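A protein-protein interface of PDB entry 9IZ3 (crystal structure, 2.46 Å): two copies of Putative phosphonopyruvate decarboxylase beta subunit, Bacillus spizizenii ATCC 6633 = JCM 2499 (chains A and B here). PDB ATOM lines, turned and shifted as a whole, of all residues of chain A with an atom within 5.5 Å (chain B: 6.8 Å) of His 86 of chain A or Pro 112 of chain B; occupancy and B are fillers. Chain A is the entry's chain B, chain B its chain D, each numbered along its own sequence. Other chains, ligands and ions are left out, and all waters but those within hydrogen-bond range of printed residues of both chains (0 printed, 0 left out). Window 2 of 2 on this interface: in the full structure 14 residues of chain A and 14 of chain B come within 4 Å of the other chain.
His 86 of chain A touches just one residue of chain B: Pro 112 (3.4 Å).
Of the printed residues of chain B, Met 83 of chain A touches Val 111.
Of the printed residues of chain A, Leu 75 of chain B touches Thr 82.
The nearest printed residue of chain B that does not touch Met 83 of chain A is Leu 75 of chain B (6.8 Å).
No position is printed for both chains.
Of the 4 pairs that touch across the chains among the printed residues, none has its exchanged pair printed and touching as well.
CG2 of Thr 82 of chain A touches CD2 of Leu 75 of chain B, at 3.7 Å.
Thr 82 of chain A touches Val 111 of chain B.
Met 83 of chain A touches Val 111 of chain B.
Pro 112 of chain B touches His 86 of chain A (CG to CD2, 3.4 Å).
Of the 9 printed residues of chain A, 3 touch a printed residue of chain B.
Hydrophobic or aromatic side chains of chain B that line the printed part of chain A: Leu 75, Val 111 and Pro 112.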
ATOM      1  N   ILE A  81     -27.512  14.105 -23.658  1.00  0.00           N
ATOM      2  CA  ILE A  81     -28.587  14.081 -22.671  1.00  0.00           C
ATOM      3  C   ILE A  81     -28.015  14.094 -21.257  1.00  0.00           C
ATOM      4  O   ILE A  81     -28.565  14.742 -20.358  1.00  0.00           O
ATOM      5  CB  ILE A  81     -29.523  12.879 -22.910  1.00  0.00           C
ATOM      6  CG1 ILE A  81     -28.814  11.551 -22.639  1.00  0.00           C
ATOM      7  CG2 ILE A  81     -30.066  12.909 -24.328  1.00  0.00           C
ATOM      8  CD1 ILE A  81     -29.725  10.356 -22.768  1.00  0.00           C
ATOM      9  N   THR A  82     -26.865  13.440 -21.054  1.00  0.00           N
ATOM     10  CA  THR A  82     -26.258  13.422 -19.727  1.00  0.00           C
ATOM     11  C   THR A  82     -25.982  14.834 -19.233  1.00  0.00           C
ATOM     12  O   THR A  82     -26.210  15.148 -18.061  1.00  0.00           O
ATOM     13  CB  THR A  82     -24.964  12.615 -19.749  1.00  0.00           C
ATOM     14  OG1 THR A  82     -24.112  13.128 -20.783  1.00  0.00           O
ATOM     15  CG2 THR A  82     -25.263  11.139 -20.002  1.00  0.00           C
ATOM     16  N   MET A  83     -25.499  15.703 -20.118  1.00  0.00           N
ATOM     17  CA  MET A  83     -25.287  17.086 -19.720  1.00  0.00           C
ATOM     18  C   MET A  83     -26.613  17.810 -19.557  1.00  0.00           C
ATOM     19  O   MET A  83     -26.812  18.539 -18.574  1.00  0.00           O
ATOM     20  CB  MET A  83     -24.381  17.771 -20.737  1.00  0.00           C
ATOM     21  CG  MET A  83     -23.061  17.037 -20.857  1.00  0.00           C
ATOM     22  SD  MET A  83     -21.894  17.711 -22.029  1.00  0.00           S
ATOM     23  CE  MET A  83     -22.803  17.584 -23.543  1.00  0.00           C
ATOM     24  N   ILE A  84     -27.559  17.577 -20.474  1.00  0.00           N
ATOM     25  CA  ILE A  84     -28.852  18.242 -20.355  1.00  0.00           C
ATOM     26  C   ILE A  84     -29.509  17.859 -19.041  1.00  0.00           C
ATOM     27  O   ILE A  84     -30.025  18.715 -18.312  1.00  0.00           O
ATOM     28  CB  ILE A  84     -29.754  17.898 -21.553  1.00  0.00           C
ATOM     29  CG1 ILE A  84     -29.139  18.380 -22.863  1.00  0.00           C
ATOM     30  CG2 ILE A  84     -31.131  18.505 -21.371  1.00  0.00           C
ATOM     31  CD1 ILE A  84     -30.017  18.053 -24.051  1.00  0.00           C
ATOM     32  N   GLY A  85     -29.473  16.567 -18.710  1.00  0.00           N
ATOM     33  CA  GLY A  85     -30.034  16.087 -17.463  1.00  0.00           C
ATOM     34  C   GLY A  85     -29.249  16.503 -16.239  1.00  0.00           C
ATOM     35  O   GLY A  85     -29.812  16.524 -15.139  1.00  0.00           O
ATOM     36  N   HIS A  86     -27.966  16.840 -16.400  1.00  0.00           N
ATOM     37  CA  HIS A  86     -27.214  17.348 -15.255  1.00  0.00           C
ATOM     38  C   HIS A  86     -27.424  18.845 -15.060  1.00  0.00           C
ATOM     39  O   HIS A  86     -27.660  19.295 -13.933  1.00  0.00           O
ATOM     40  CB  HIS A  86     -25.721  17.049 -15.408  1.00  0.00           C
ATOM     41  CG  HIS A  86     -24.903  17.437 -14.214  1.00  0.00           C
ATOM     42  ND1 HIS A  86     -23.786  18.239 -14.302  1.00  0.00           N
ATOM     43  CD2 HIS A  86     -25.051  17.139 -12.901  1.00  0.00           C
ATOM     44  CE1 HIS A  86     -23.277  18.412 -13.096  1.00  0.00           C
ATOM     45  NE2 HIS A  86     -24.024  17.755 -12.228  1.00  0.00           N
ATOM     46  N   GLN A  87     -27.350  19.623 -16.143  1.00  0.00           N
ATOM     47  CA  GLN A  87     -27.562  21.065 -16.042  1.00  0.00           C
ATOM     48  C   GLN A  87     -29.002  21.400 -15.675  1.00  0.00           C
ATOM     49  O   GLN A  87     -29.251  22.404 -15.000  1.00  0.00           O
ATOM     50  CB  GLN A  87     -27.178  21.732 -17.360  1.00  0.00           C
ATOM     51  CG  GLN A  87     -25.683  21.695 -17.653  1.00  0.00           C
ATOM     52  CD  GLN A  87     -24.911  22.688 -16.808  1.00  0.00           C
ATOM     53  OE1 GLN A  87     -25.236  23.876 -16.775  1.00  0.00           O
ATOM     54  NE2 GLN A  87     -23.886  22.206 -16.116  1.00  0.00           N
ATOM     55  N   LYS A  88     -29.952  20.571 -16.099  1.00  0.00           N
ATOM     56  CA  LYS A  88     -31.369  20.763 -15.835  1.00  0.00           C
ATOM     57  C   LYS A  88     -31.886  22.152 -16.194  1.00  0.00           C
ATOM     58  O   LYS A  88     -32.387  22.887 -15.329  1.00  0.00           O
ATOM     59  CB  LYS A  88     -31.676  20.445 -14.365  1.00  0.00           C
ATOM     60  CG  LYS A  88     -31.476  18.987 -14.004  1.00  0.00           C
ATOM     61  CD  LYS A  88     -32.253  18.593 -12.761  1.00  0.00           C
ATOM     62  CE  LYS A  88     -32.153  17.090 -12.521  1.00  0.00           C
ATOM     63  NZ  LYS A  88     -30.736  16.642 -12.408  1.00  0.00           N
ATOM     64  N   VAL A 123     -31.496   9.964 -16.940  1.00  0.00           N
ATOM     65  CA  VAL A 123     -30.363  10.888 -16.868  1.00  0.00           C
ATOM     66  C   VAL A 123     -30.710  12.224 -16.231  1.00  0.00           C
ATOM     67  O   VAL A 123     -29.841  13.102 -16.154  1.00  0.00           O
ATOM     68  CB  VAL A 123     -29.765  11.157 -18.261  1.00  0.00           C
ATOM     69  CG1 VAL A 123     -29.335   9.846 -18.906  1.00  0.00           C
ATOM     70  CG2 VAL A 123     -30.773  11.900 -19.125  1.00  0.00           C
ATOM     71  N   ASP B  71     -15.742   5.907 -16.340  1.00  0.00           N
ATOM     72  CA  ASP B  71     -16.904   6.778 -16.490  1.00  0.00           C
ATOM     73  C   ASP B  71     -16.678   7.800 -17.597  1.00  0.00           C
ATOM     74  O   ASP B  71     -17.586   8.083 -18.386  1.00  0.00           O
ATOM     75  CB  ASP B  71     -17.218   7.474 -15.168  1.00  0.00           C
ATOM     76  CG  ASP B  71     -15.982   8.025 -14.490  1.00  0.00           C
ATOM     77  OD1 ASP B  71     -15.018   7.257 -14.291  1.00  0.00           O
ATOM     78  OD2 ASP B  71     -15.977   9.228 -14.151  1.00  0.00           O
ATOM     79  N   LEU B  75     -18.864   7.832 -20.984  1.00  0.00           N
ATOM     80  CA  LEU B  75     -19.661   8.993 -21.363  1.00  0.00           C
ATOM     81  C   LEU B  75     -19.228   9.560 -22.708  1.00  0.00           C
ATOM     82  O   LEU B  75     -20.065  10.052 -23.472  1.00  0.00           O
ATOM     83  CB  LEU B  75     -19.564  10.066 -20.279  1.00  0.00           C
ATOM     84  CG  LEU B  75     -20.373   9.841 -19.002  1.00  0.00           C
ATOM     85  CD1 LEU B  75     -19.951  10.833 -17.937  1.00  0.00           C
ATOM     86  CD2 LEU B  75     -21.859   9.966 -19.279  1.00  0.00           C
ATOM     87  N   ASP B  98     -15.857   3.659 -12.185  1.00  0.00           N
ATOM     88  CA  ASP B  98     -16.319   5.032 -12.060  1.00  0.00           C
ATOM     89  C   ASP B  98     -15.801   5.654 -10.771  1.00  0.00           C
ATOM     90  O   ASP B  98     -15.787   5.008  -9.719  1.00  0.00           O
ATOM     91  CB  ASP B  98     -17.852   5.079 -12.099  1.00  0.00           C
ATOM     92  CG  ASP B  98     -18.412   6.480 -11.937  1.00  0.00           C
ATOM     93  OD1 ASP B  98     -17.653   7.466 -12.053  1.00  0.00           O
ATOM     94  OD2 ASP B  98     -19.632   6.593 -11.696  1.00  0.00           O
ATOM     95  N   ARG B 109     -17.484  19.505 -11.488  1.00  0.00           N
ATOM     96  CA  ARG B 109     -16.148  18.993 -11.769  1.00  0.00           C
ATOM     97  C   ARG B 109     -16.153  18.156 -13.041  1.00  0.00           C
ATOM     98  O   ARG B 109     -15.356  18.378 -13.951  1.00  0.00           O
ATOM     99  CB  ARG B 109     -15.629  18.167 -10.592  1.00  0.00           C
ATOM    100  CG  ARG B 109     -14.248  17.570 -10.807  1.00  0.00           C
ATOM    101  CD  ARG B 109     -13.204  18.641 -11.079  1.00  0.00           C
ATOM    102  NE  ARG B 109     -11.897  18.055 -11.362  1.00  0.00           N
ATOM    103  CZ  ARG B 109     -11.541  17.585 -12.551  1.00  0.00           C
ATOM    104  NH1 ARG B 109     -10.337  17.062 -12.739  1.00  0.00           N
ATOM    105  NH2 ARG B 109     -12.401  17.637 -13.554  1.00  0.00           N
ATOM    106  N   THR B 110     -17.071  17.196 -13.090  1.00  0.00           N
ATOM    107  CA  THR B 110     -17.200  16.285 -14.213  1.00  0.00           C
ATOM    108  C   THR B 110     -18.680  16.011 -14.438  1.00  0.00           C
ATOM    109  O   THR B 110     -19.515  16.260 -13.564  1.00  0.00           O
ATOM    110  CB  THR B 110     -16.430  14.975 -13.962  1.00  0.00           C
ATOM    111  OG1 THR B 110     -16.543  14.114 -15.101  1.00  0.00           O
ATOM    112  CG2 THR B 110     -16.972  14.258 -12.727  1.00  0.00           C
ATOM    113  N   VAL B 111     -19.005  15.515 -15.627  1.00  0.00           N
ATOM    114  CA  VAL B 111     -20.373  15.086 -15.904  1.00  0.00           C
ATOM    115  C   VAL B 111     -20.598  13.778 -15.156  1.00  0.00           C
ATOM    116  O   VAL B 111     -19.882  12.794 -15.398  1.00  0.00           O
ATOM    117  CB  VAL B 111     -20.629  14.933 -17.411  1.00  0.00           C
ATOM    118  CG1 VAL B 111     -22.002  14.328 -17.655  1.00  0.00           C
ATOM    119  CG2 VAL B 111     -20.515  16.282 -18.100  1.00  0.00           C
ATOM    120  N   PRO B 112     -21.553  13.720 -14.233  1.00  0.00           N
ATOM    121  CA  PRO B 112     -21.746  12.493 -13.449  1.00  0.00           C
ATOM    122  C   PRO B 112     -22.438  11.402 -14.253  1.00  0.00           C
ATOM    123  O   PRO B 112     -23.371  11.660 -15.019  1.00  0.00           O
ATOM    124  CB  PRO B 112     -22.619  12.959 -12.279  1.00  0.00           C
ATOM    125  CG  PRO B 112     -23.385  14.125 -12.831  1.00  0.00           C
ATOM    126  CD  PRO B 112     -22.475  14.797 -13.830  1.00  0.00           C
ATOM    127  N   LEU B 113     -21.961  10.172 -14.073  1.00  0.00           N
ATOM    128  CA  LEU B 113     -22.583   8.992 -14.666  1.00  0.00           C
ATOM    129  C   LEU B 113     -23.708   8.528 -13.750  1.00  0.00           C
ATOM    130  O   LEU B 113     -23.459   8.098 -12.620  1.00  0.00           O
ATOM    131  CB  LEU B 113     -21.549   7.889 -14.866  1.00  0.00           C
ATOM    132  CG  LEU B 113     -22.042   6.620 -15.562  1.00  0.00           C
ATOM    133  CD1 LEU B 113     -22.608   6.950 -16.932  1.00  0.00           C
ATOM    134  CD2 LEU B 113     -20.913   5.608 -15.676  1.00  0.00           C
ATOM    135  N   VAL B 114     -24.947   8.604 -14.233  1.00  0.00           N
ATOM    136  CA  VAL B 114     -26.132   8.413 -13.405  1.00  0.00           C
ATOM    137  C   VAL B 114     -26.960   7.266 -13.971  1.00  0.00           C
ATOM    138  O   VAL B 114     -27.238   7.229 -15.175  1.00  0.00           O
ATOM    139  CB  VAL B 114     -26.971   9.703 -13.327  1.00  0.00           C
ATOM    140  CG1 VAL B 114     -28.145   9.518 -12.389  1.00  0.00           C
ATOM    141  CG2 VAL B 114     -26.103  10.865 -12.878  1.00  0.00           C
